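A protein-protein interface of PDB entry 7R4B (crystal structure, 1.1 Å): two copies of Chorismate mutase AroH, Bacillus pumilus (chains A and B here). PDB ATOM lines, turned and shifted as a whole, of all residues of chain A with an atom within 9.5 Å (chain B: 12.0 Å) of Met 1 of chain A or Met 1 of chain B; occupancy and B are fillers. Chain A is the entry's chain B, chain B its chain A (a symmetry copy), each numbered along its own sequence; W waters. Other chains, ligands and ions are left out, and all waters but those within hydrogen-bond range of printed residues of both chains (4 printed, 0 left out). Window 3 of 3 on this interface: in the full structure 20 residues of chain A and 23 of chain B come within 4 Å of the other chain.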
ATOM      1  N   MET A   1      22.450   0.617  -3.297  1.00  0.00           N
ATOM      2  CA  MET A   1      23.094   1.712  -2.567  1.00  0.00           C
ATOM      3  C   MET A   1      23.287   1.282  -1.144  1.00  0.00           C
ATOM      4  O   MET A   1      22.630   0.364  -0.662  1.00  0.00           O
ATOM      5  CB  MET A   1      22.230   2.977  -2.550  1.00  0.00           C
ATOM      6  CG  MET A   1      21.581   3.308  -3.856  1.00  0.00           C
ATOM      7  SD  MET A   1      20.932   4.988  -3.945  1.00  0.00           S
ATOM      8  CE  MET A   1      21.943   5.919  -2.794  1.00  0.00           C
ATOM      9  N   MET A   2      24.166   1.982  -0.461  1.00  0.00           N
ATOM     10  CA  MET A   2      24.378   1.818   0.966  1.00  0.00           C
ATOM     11  C   MET A   2      23.255   2.557   1.722  1.00  0.00           C
ATOM     12  O   MET A   2      22.485   3.338   1.158  1.00  0.00           O
ATOM     13  CB  MET A   2      25.776   2.346   1.295  1.00  0.00           C
ATOM     14  CG  MET A   2      26.229   2.190   2.736  1.00  0.00           C
ATOM     15  SD  MET A   2      26.053   0.492   3.349  1.00  0.00           S
ATOM     16  CE  MET A   2      26.740   0.716   4.973  1.00  0.00           C
ATOM     17  N   PHE A   3      23.160   2.265   3.009  1.00  0.00           N
ATOM     18  CA  PHE A   3      22.217   2.886   3.926  1.00  0.00           C
ATOM     19  C   PHE A   3      22.985   3.352   5.149  1.00  0.00           C
ATOM     20  O   PHE A   3      23.988   2.737   5.549  1.00  0.00           O
ATOM     21  CB  PHE A   3      21.120   1.878   4.337  1.00  0.00           C
ATOM     22  CG  PHE A   3      20.130   1.617   3.233  1.00  0.00           C
ATOM     23  CD1 PHE A   3      20.481   0.847   2.134  1.00  0.00           C
ATOM     24  CD2 PHE A   3      18.872   2.188   3.260  1.00  0.00           C
ATOM     25  CE1 PHE A   3      19.573   0.644   1.096  1.00  0.00           C
ATOM     26  CE2 PHE A   3      17.977   1.996   2.247  1.00  0.00           C
ATOM     27  CZ  PHE A   3      18.330   1.240   1.142  1.00  0.00           C
ATOM     28  N   ARG A   4      22.524   4.458   5.735  1.00  0.00           N
ATOM     29  CA  ARG A   4      23.236   5.078   6.826  1.00  0.00           C
ATOM     30  C   ARG A   4      22.260   5.613   7.860  1.00  0.00           C
ATOM     31  O   ARG A   4      21.218   6.184   7.519  1.00  0.00           O
ATOM     32  CB  ARG A   4      24.065   6.279   6.342  1.00  0.00           C
ATOM     33  CG  ARG A   4      25.189   5.963   5.387  1.00  0.00           C
ATOM     34  CD  ARG A   4      26.280   5.225   6.069  1.00  0.00           C
ATOM     35  NE  ARG A   4      27.332   4.795   5.159  1.00  0.00           N
ATOM     36  CZ  ARG A   4      28.270   3.918   5.484  1.00  0.00           C
ATOM     37  NH1 ARG A   4      28.343   3.414   6.696  1.00  0.00           N
ATOM     38  NH2 ARG A   4      29.130   3.502   4.556  1.00  0.00           N
ATOM     39  N   ARG A  41      13.483   8.089   0.402  1.00  0.00           N
ATOM     40  CA  ARG A  41      14.721   7.382   0.725  1.00  0.00           C
ATOM     41  C   ARG A  41      14.875   7.069   2.208  1.00  0.00           C
ATOM     42  O   ARG A  41      15.895   6.477   2.590  1.00  0.00           O
ATOM     43  CB  ARG A  41      15.936   8.183   0.239  1.00  0.00           C
ATOM     44  CG  ARG A  41      16.070   8.105  -1.278  1.00  0.00           C
ATOM     45  CD  ARG A  41      17.406   8.675  -1.750  1.00  0.00           C
ATOM     46  NE  ARG A  41      17.437  10.110  -1.510  1.00  0.00           N
ATOM     47  CZ  ARG A  41      18.100  10.720  -0.537  1.00  0.00           C
ATOM     48  NH1 ARG A  41      18.943  10.074   0.251  1.00  0.00           N
ATOM     49  NH2 ARG A  41      17.907  12.012  -0.344  1.00  0.00           N
ATOM     50  N   VAL A  43      14.086   4.869   5.268  1.00  0.00           N
ATOM     51  CA  VAL A  43      13.573   3.569   5.679  1.00  0.00           C
ATOM     52  C   VAL A  43      12.620   3.720   6.853  1.00  0.00           C
ATOM     53  O   VAL A  43      11.510   3.175   6.853  1.00  0.00           O
ATOM     54  CB  VAL A  43      14.746   2.632   6.033  1.00  0.00           C
ATOM     55  CG1 VAL A  43      14.233   1.275   6.531  1.00  0.00           C
ATOM     56  CG2 VAL A  43      15.698   2.486   4.859  1.00  0.00           C
ATOM     57  N   VAL A  95      18.580   6.132   6.240  1.00  0.00           N
ATOM     58  CA  VAL A  95      18.425   6.718   4.908  1.00  0.00           C
ATOM     59  C   VAL A  95      19.264   5.972   3.875  1.00  0.00           C
ATOM     60  O   VAL A  95      20.427   5.623   4.128  1.00  0.00           O
ATOM     61  CB  VAL A  95      18.828   8.213   4.924  1.00  0.00           C
ATOM     62  CG1 VAL A  95      18.539   8.912   3.582  1.00  0.00           C
ATOM     63  CG2 VAL A  95      18.153   8.957   6.068  1.00  0.00           C
ATOM     64  N   GLN A  96      18.678   5.780   2.680  1.00  0.00           N
ATOM     65  CA  GLN A  96      19.418   5.266   1.532  1.00  0.00           C
ATOM     66  C   GLN A  96      20.346   6.374   1.036  1.00  0.00           C
ATOM     67  O   GLN A  96      19.876   7.446   0.639  1.00  0.00           O
ATOM     68  CB  GLN A  96      18.428   4.901   0.432  1.00  0.00           C
ATOM     69  CG  GLN A  96      19.037   4.178  -0.748  1.00  0.00           C
ATOM     70  CD  GLN A  96      18.040   4.048  -1.893  1.00  0.00           C
ATOM     71  OE1 GLN A  96      17.300   4.986  -2.201  1.00  0.00           O
ATOM     72  NE2 GLN A  96      17.991   2.876  -2.501  1.00  0.00           N
ATOM     73  N   THR A  97      21.659   6.145   1.107  1.00  0.00           N
ATOM     74  CA  THR A  97      22.627   7.129   0.647  1.00  0.00           C
ATOM     75  C   THR A  97      23.975   6.461   0.454  1.00  0.00           C
ATOM     76  O   THR A  97      24.358   5.594   1.239  1.00  0.00           O
ATOM     77  CB  THR A  97      22.757   8.275   1.660  1.00  0.00           C
ATOM     78  OG1 THR A  97      23.739   9.200   1.178  1.00  0.00           O
ATOM     79  CG2 THR A  97      23.204   7.796   3.036  1.00  0.00           C
ATOM     80  N   ASP A  98      24.697   6.894  -0.584  1.00  0.00           N
ATOM     81  CA  ASP A  98      26.076   6.486  -0.798  1.00  0.00           C
ATOM     82  C   ASP A  98      27.079   7.461  -0.177  1.00  0.00           C
ATOM     83  O   ASP A  98      28.280   7.309  -0.399  1.00  0.00           O
ATOM     84  CB  ASP A  98      26.367   6.255  -2.286  1.00  0.00           C
ATOM     85  CG  ASP A  98      25.870   4.897  -2.783  1.00  0.00           C
ATOM     86  OD1 ASP A  98      25.708   3.951  -1.979  1.00  0.00           O
ATOM     87  OD2 ASP A  98      25.656   4.758  -4.008  1.00  0.00           O
ATOM     88  N   THR A  99      26.624   8.475   0.553  1.00  0.00           N
ATOM     89  CA  THR A  99      27.543   9.360   1.264  1.00  0.00           C
ATOM     90  C   THR A  99      28.441   8.554   2.195  1.00  0.00           C
ATOM     91  O   THR A  99      27.985   7.659   2.912  1.00  0.00           O
ATOM     92  CB  THR A  99      26.727  10.396   2.045  1.00  0.00           C
ATOM     93  OG1 THR A  99      26.026  11.235   1.105  1.00  0.00           O
ATOM     94  CG2 THR A  99      27.605  11.230   2.969  1.00  0.00           C
ATOM     95  N   MET B   1      23.699  -6.020  -2.189  1.00  0.00           N
ATOM     96  CA  MET B   1      24.007  -5.296  -0.927  1.00  0.00           C
ATOM     97  C   MET B   1      22.884  -5.384   0.135  1.00  0.00           C
ATOM     98  O   MET B   1      22.045  -4.497   0.246  1.00  0.00           O
ATOM     99  CB  MET B   1      24.311  -3.816  -1.238  1.00  0.00           C
ATOM    100  CG  MET B   1      25.071  -3.122  -0.121  1.00  0.00           C
ATOM    101  SD  MET B   1      25.893  -1.572  -0.506  1.00  0.00           S
ATOM    102  CE  MET B   1      27.314  -2.202  -1.477  1.00  0.00           C
ATOM    103  N   MET B   2      22.895  -6.455   0.914  1.00  0.00           N
ATOM    104  CA  MET B   2      21.858  -6.759   1.889  1.00  0.00           C
ATOM    105  C   MET B   2      22.292  -6.291   3.269  1.00  0.00           C
ATOM    106  O   MET B   2      23.461  -5.970   3.497  1.00  0.00           O
ATOM    107  CB  MET B   2      21.560  -8.262   1.862  1.00  0.00           C
ATOM    108  CG  MET B   2      20.398  -8.727   2.718  1.00  0.00           C
ATOM    109  SD  MET B   2      18.863  -7.809   2.488  1.00  0.00           S
ATOM    110  CE  MET B   2      17.794  -8.610   3.659  1.00  0.00           C
ATOM    111  N   PHE B   3      21.307  -6.183   4.172  1.00  0.00           N
ATOM    112  CA  PHE B   3      21.543  -5.782   5.559  1.00  0.00           C
ATOM    113  C   PHE B   3      20.904  -6.791   6.503  1.00  0.00           C
ATOM    114  O   PHE B   3      19.874  -7.392   6.174  1.00  0.00           O
ATOM    115  CB  PHE B   3      20.984  -4.369   5.832  1.00  0.00           C
ATOM    116  CG  PHE B   3      21.621  -3.335   4.973  1.00  0.00           C
ATOM    117  CD1 PHE B   3      22.667  -2.564   5.452  1.00  0.00           C
ATOM    118  CD2 PHE B   3      21.216  -3.165   3.665  1.00  0.00           C
ATOM    119  CE1 PHE B   3      23.303  -1.650   4.640  1.00  0.00           C
ATOM    120  CE2 PHE B   3      21.839  -2.242   2.844  1.00  0.00           C
ATOM    121  CZ  PHE B   3      22.890  -1.479   3.336  1.00  0.00           C
ATOM    122  N   ARG B   4      21.519  -6.960   7.674  1.00  0.00           N
ATOM    123  CA  ARG B   4      21.040  -7.887   8.680  1.00  0.00           C
ATOM    124  C   ARG B   4      21.182  -7.263  10.060  1.00  0.00           C
ATOM    125  O   ARG B   4      22.207  -6.650  10.383  1.00  0.00           O
ATOM    126  CB  ARG B   4      21.847  -9.195   8.654  1.00  0.00           C
ATOM    127  CG  ARG B   4      21.756  -9.975   7.358  1.00  0.00           C
ATOM    128  CD  ARG B   4      20.367 -10.553   7.173  1.00  0.00           C
ATOM    129  NE  ARG B   4      20.177 -11.140   5.851  1.00  0.00           N
ATOM    130  CZ  ARG B   4      19.001 -11.540   5.408  1.00  0.00           C
ATOM    131  NH1 ARG B   4      17.919 -11.415   6.152  1.00  0.00           N
ATOM    132  NH2 ARG B   4      18.906 -12.059   4.188  1.00  0.00           N
ATOM    133  N   GLY B   5      20.174  -7.471  10.904  1.00  0.00           N
ATOM    134  CA  GLY B   5      20.328  -7.164  12.319  1.00  0.00           C
ATOM    135  C   GLY B   5      21.112  -8.270  13.012  1.00  0.00           C
ATOM    136  O   GLY B   5      20.927  -9.463  12.739  1.00  0.00           O
ATOM    137  N   ASP B  38      33.140  -4.805   9.846  1.00  0.00           N
ATOM    138  CA  ASP B  38      33.878  -3.579   9.547  1.00  0.00           C
ATOM    139  C   ASP B  38      33.006  -2.400   9.951  1.00  0.00           C
ATOM    140  O   ASP B  38      31.838  -2.335   9.516  1.00  0.00           O
ATOM    141  CB  ASP B  38      34.135  -3.549   8.039  1.00  0.00           C
ATOM    142  CG  ASP B  38      34.896  -2.324   7.561  1.00  0.00           C
ATOM    143  OD1 ASP B  38      34.967  -1.289   8.254  1.00  0.00           O
ATOM    144  OD2 ASP B  38      35.392  -2.393   6.413  1.00  0.00           O
ATOM    145  N   GLU B  40      32.771   0.515   8.952  1.00  0.00           N
ATOM    146  CA  GLU B  40      32.269   1.278   7.816  1.00  0.00           C
ATOM    147  C   GLU B  40      31.032   0.640   7.185  1.00  0.00           C
ATOM    148  O   GLU B  40      30.281   1.332   6.480  1.00  0.00           O
ATOM    149  CB  GLU B  40      33.422   1.445   6.821  1.00  0.00           C
ATOM    150  CG  GLU B  40      33.130   2.338   5.645  1.00  0.00           C
ATOM    151  CD  GLU B  40      32.380   1.634   4.537  1.00  0.00           C
ATOM    152  OE1 GLU B  40      31.630   2.327   3.818  1.00  0.00           O
ATOM    153  OE2 GLU B  40      32.545   0.391   4.386  1.00  0.00           O
ATOM    154  N   ARG B  41      30.779  -0.641   7.452  1.00  0.00           N
ATOM    155  CA  ARG B  41      29.601  -1.354   6.956  1.00  0.00           C
ATOM    156  C   ARG B  41      28.437  -1.344   7.939  1.00  0.00           C
ATOM    157  O   ARG B  41      27.401  -1.952   7.665  1.00  0.00           O
ATOM    158  CB  ARG B  41      29.990  -2.801   6.641  1.00  0.00           C
ATOM    159  CG  ARG B  41      31.007  -2.952   5.506  1.00  0.00           C
ATOM    160  CD  ARG B  41      30.366  -2.709   4.150  1.00  0.00           C
ATOM    161  NE  ARG B  41      30.318  -1.294   3.801  1.00  0.00           N
ATOM    162  CZ  ARG B  41      29.592  -0.790   2.813  1.00  0.00           C
ATOM    163  NH1 ARG B  41      28.778  -1.548   2.104  1.00  0.00           N
ATOM    164  NH2 ARG B  41      29.688   0.505   2.529  1.00  0.00           N
ATOM    165  N   VAL B  42      28.567  -0.657   9.057  1.00  0.00           N
ATOM    166  CA  VAL B  42      27.517  -0.639  10.068  1.00  0.00           C
ATOM    167  C   VAL B  42      26.628   0.574   9.851  1.00  0.00           C
ATOM    168  O   VAL B  42      27.097   1.721   9.923  1.00  0.00           O
ATOM    169  CB  VAL B  42      28.091  -0.632  11.487  1.00  0.00           C
ATOM    170  CG1 VAL B  42      26.976  -0.593  12.527  1.00  0.00           C
ATOM    171  CG2 VAL B  42      28.974  -1.865  11.700  1.00  0.00           C
ATOM    172  N   VAL B  43      25.339   0.321   9.618  1.00  0.00           N
ATOM    173  CA  VAL B  43      24.363   1.390   9.412  1.00  0.00           C
ATOM    174  C   VAL B  43      24.146   2.162  10.702  1.00  0.00           C
ATOM    175  O   VAL B  43      24.163   3.399  10.713  1.00  0.00           O
ATOM    176  CB  VAL B  43      23.046   0.783   8.904  1.00  0.00           C
ATOM    177  CG1 VAL B  43      21.990   1.864   8.752  1.00  0.00           C
ATOM    178  CG2 VAL B  43      23.264   0.038   7.600  1.00  0.00           C
ATOM    179  N   THR B  94      22.911  -3.090  13.045  1.00  0.00           N
ATOM    180  CA  THR B  94      22.441  -3.272  11.672  1.00  0.00           C
ATOM    181  C   THR B  94      23.641  -3.167  10.751  1.00  0.00           C
ATOM    182  O   THR B  94      24.261  -2.107  10.666  1.00  0.00           O
ATOM    183  CB  THR B  94      21.390  -2.230  11.293  1.00  0.00           C
ATOM    184  OG1 THR B  94      20.309  -2.275  12.234  1.00  0.00           O
ATOM    185  CG2 THR B  94      20.845  -2.503   9.921  1.00  0.00           C
ATOM    186  N   VAL B  95      23.964  -4.259  10.069  1.00  0.00           N
ATOM    187  CA  VAL B  95      25.211  -4.388   9.323  1.00  0.00           C
ATOM    188  C   VAL B  95      24.905  -4.725   7.872  1.00  0.00           C
ATOM    189  O   VAL B  95      24.022  -5.536   7.577  1.00  0.00           O
ATOM    190  CB  VAL B  95      26.103  -5.484   9.936  1.00  0.00           C
ATOM    191  CG1 VAL B  95      27.413  -5.624   9.172  1.00  0.00           C
ATOM    192  CG2 VAL B  95      26.361  -5.215  11.400  1.00  0.00           C
ATOM    193  N   GLN B  96      25.681  -4.137   6.966  1.00  0.00           N
ATOM    194  CA  GLN B  96      25.665  -4.524   5.563  1.00  0.00           C
ATOM    195  C   GLN B  96      26.462  -5.812   5.444  1.00  0.00           C
ATOM    196  O   GLN B  96      27.693  -5.804   5.580  1.00  0.00           O
ATOM    197  CB  GLN B  96      26.264  -3.419   4.696  1.00  0.00           C
ATOM    198  CG  GLN B  96      25.912  -3.561   3.223  1.00  0.00           C
ATOM    199  CD  GLN B  96      26.787  -4.567   2.542  1.00  0.00           C
ATOM    200  OE1 GLN B  96      27.977  -4.323   2.284  1.00  0.00           O
ATOM    201  NE2 GLN B  96      26.207  -5.716   2.220  1.00  0.00           N
ATOM    202  N   THR B  97      25.761  -6.924   5.239  1.00  0.00           N
ATOM    203  CA  THR B  97      26.395  -8.218   5.090  1.00  0.00           C
ATOM    204  C   THR B  97      25.557  -9.081   4.170  1.00  0.00           C
ATOM    205  O   THR B  97      24.327  -8.985   4.153  1.00  0.00           O
ATOM    206  CB  THR B  97      26.583  -8.937   6.429  1.00  0.00           C
ATOM    207  OG1 THR B  97      27.118 -10.242   6.167  1.00  0.00           O
ATOM    208  CG2 THR B  97      25.261  -9.103   7.185  1.00  0.00           C
ATOM    209  N   ASP B  98      26.254  -9.918   3.410  1.00  0.00           N
ATOM    210  CA  ASP B  98      25.669 -10.875   2.487  1.00  0.00           C
ATOM    211  C   ASP B  98      25.459 -12.257   3.100  1.00  0.00           C
ATOM    212  O   ASP B  98      25.044 -13.170   2.389  1.00  0.00           O
ATOM    213  CB  ASP B  98      26.587 -11.038   1.254  1.00  0.00           C
ATOM    214  CG  ASP B  98      27.977 -11.659   1.601  1.00  0.00           C
ATOM    215  OD1 ASP B  98      28.388 -11.636   2.786  1.00  0.00           O
ATOM    216  OD2 ASP B  98      28.656 -12.197   0.690  1.00  0.00           O
ATOM    217  N   THR B  99      25.767 -12.445   4.377  1.00  0.00           N
ATOM    218  CA  THR B  99      25.597 -13.743   5.016  1.00  0.00           C
ATOM    219  C   THR B  99      24.119 -14.134   5.014  1.00  0.00           C
ATOM    220  O   THR B  99      23.234 -13.292   5.191  1.00  0.00           O
ATOM    221  CB  THR B  99      26.104 -13.634   6.459  1.00  0.00           C
ATOM    222  OG1 THR B  99      27.472 -13.195   6.475  1.00  0.00           O
ATOM    223  CG2 THR B  99      26.019 -14.966   7.164  1.00  0.00           C
ATOM    224  N   LYS B 100      23.846 -15.425   4.826  1.00  0.00           N
ATOM    225  CA  LYS B 100      22.474 -15.901   4.898  1.00  0.00           C
ATOM    226  C   LYS B 100      21.902 -15.575   6.269  1.00  0.00           C
ATOM    227  O   LYS B 100      22.609 -15.603   7.278  1.00  0.00           O
ATOM    228  CB  LYS B 100      22.406 -17.420   4.701  1.00  0.00           C
ATOM    229  CG  LYS B 100      22.833 -17.951   3.333  1.00  0.00           C
ATOM    230  CD  LYS B 100      22.669 -19.484   3.269  1.00  0.00           C
ATOM    231  CE  LYS B 100      22.468 -20.022   1.852  1.00  0.00           C
ATOM    232  NZ  LYS B 100      22.245 -21.509   1.803  1.00  0.00           N
ATOM    233  N   GLN B 101      20.593 -15.309   6.304  1.00  0.00           N
ATOM    234  CA  GLN B 101      19.949 -14.880   7.546  1.00  0.00           C
ATOM    235  C   GLN B 101      20.225 -15.867   8.679  1.00  0.00           C
ATOM    236  O   GLN B 101      20.563 -15.476   9.806  1.00  0.00           O
ATOM    237  CB  GLN B 101      18.445 -14.735   7.325  1.00  0.00           C
ATOM    238  CG  GLN B 101      17.709 -14.295   8.560  1.00  0.00           C
ATOM    239  CD  GLN B 101      16.223 -14.209   8.331  1.00  0.00           C
ATOM    240  OE1 GLN B 101      15.557 -15.218   8.109  1.00  0.00           O
ATOM    241  NE2 GLN B 101      15.698 -12.995   8.343  1.00  0.00           N
HETATM  242  O   HOH W   1      21.184  -2.061  -0.856  1.00  0.00           O
HETATM  243  O   HOH W   2      24.515  -0.979  -3.268  1.00  0.00           O
HETATM  244  O   HOH W   3      27.006   4.264   9.141  1.00  0.00           O
HETATM  245  O   HOH W   4      32.032   5.128   3.928  1.00  0.00           O
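SD of Met 2 of chain A sits at hydrogen-bond distance from NH1 of Arg 41 of chain B. The backbone carbonyl oxygen (O) of Met 1 of chain A sits close to the side-chain sulfur (SD) of Met 1 of chain B (3.8 Å). NH2 of Arg 4 of chain A lies within salt-bridge range of OE1 of Glu 40 of chain B, 2.9 Å away.
OE2 of Glu 40 of chain B is in salt-bridge range of NE of Arg 41 of chain B (2.9 Å). The backbone NH (N) of Thr 97 of chain A is in hydrogen-bond range of the backbone carbonyl oxygen (O) of Met 2 of chain A. N of Val 43 of chain B lies within hydrogen-bond range of O of Thr 94 of chain B, at 2.9 Å. The backbone carbonyl oxygen (O) of Arg 41 of chain B lies within hydrogen-bond range of the backbone NH (N) of Gln 96 of chain B, at 2.9 Å. OD1 of Asp 38 of chain B sits at hydrogen-bond distance from N of Glu 40 of chain B (2.9 Å). N of Arg 4 of chain A is in hydrogen-bond range of O of Val 95 of chain A (2.9 Å).
Met 2 of chain A touches Met 1 of chain B (N to SD, 3.95 Å). SD of Met 2 of chain A touches CE1 of Phe 3 of chain B, 3.7 Å away. Glu 40 of chain B touches Met 2 of chain A (O to CE, 3.9 Å). Phe 3 of chain B touches Phe 3 of chain A (CE2 to CD1, 3.4 Å). Val 43 of chain B touches Phe 3 of chain A (CG2 to O, 3.5 Å). Arg 4 of chain A touches Arg 41 of chain B. NH1 of Arg 4 of chain A touches O of Val 42 of chain B, 3.9 Å away. Arg 4 of chain A touches Val 43 of chain B.
Of chain B, only Met 1 comes within 4 Å of Met 1 of chain A. Printed residues of chain B within 4 Å of Met 2 of chain A: Met 1 (3.95 Å), Phe 3 (3.7 Å), Glu 40 (3.9 Å) and Arg 41 (3.6 Å). No residue of chain B comes within 4 Å of Thr 97 of chain A. No residue of chain B comes within 4 Å of Asp 98 of chain A. Met 1 of chain B touches two residues of chain A. Of the printed residues of chain A, Phe 3 of chain B touches Met 2 and Phe 3. Of the printed residues of chain A, Glu 40 of chain B touches Met 2 and Arg 4. Printed residues of chain A within 4 Å of Arg 41 of chain B: Met 2 (3.6 Å) and Arg 4 (3.7 Å). Of the printed residues of chain A, Val 42 of chain B touches Arg 4 (3.9 Å). Printed residues of chain A within 4 Å of Val 43 of chain B: Phe 3 and Arg 4. The nearest residue of chain B that does not touch Met 1 of chain A is Phe 3 of chain B (4.4 Å).
Printed residues of chain A that touch a printed residue of chain B: Met 1, Met 2, Phe 3 and Arg 4. Along chain A the printed residues that touch a printed residue of chain B span positions 1 to 4. Of the 18 printed residues of chain B, 6 touch a printed residue of chain A. Printed residues of chain B that touch a printed residue of chain A: Met 1, Phe 3, Glu 40, Arg 41, Val 42 and Val 43. Hydrophobic or aromatic side chains of chain B within 4 Å of the printed part of chain A: Met 1, Phe 3 and Val 43.
Met 2 of chain A touches Met 1 of chain B, but with the chains exchanged Met 1 of chain A does not touch Met 2 of chain B (7.0 Å). Met 2 of chain A touches Arg 41 of chain B, but with the chains exchanged Arg 41 of chain A does not touch Met 2 of chain B (14.3 Å). Phe 3 of chain A touches Val 43 of chain B, but with the chains exchanged Val 43 of chain A does not touch Phe 3 of chain B (8.0 Å). Arg 4 of chain A touches Arg 41 of chain B, but with the chains exchanged Arg 41 of chain A does not touch Arg 4 of chain B (15.4 Å). Of the 11 pairs that touch across the chains among the printed residues, 2 have their exchanged pair printed and touching as well.
Water W2 bridges the backbone NH (N) of Met 1 of chain A (2.6 Å) and the side-chain sulfur (SD) of Met 1 of chain B (3.1 Å). Water W3 lies within hydrogen-bond range of O of Val 42 of chain B, NH1 of Arg 4 of chain A and O of Val 43 of chain B. Water W1 lies within hydrogen-bond range of the backbone carbonyl oxygen of Met 1 of chain B and the backbone carbonyl oxygen of Met 1 of chain A. Water W4 lies within hydrogen-bond range of the side-chain carboxylate (OE1) of Glu 40 of chain B (2.8 Å) and the guanidinium group (NH2) of Arg 4 of chain A (3.4 Å).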
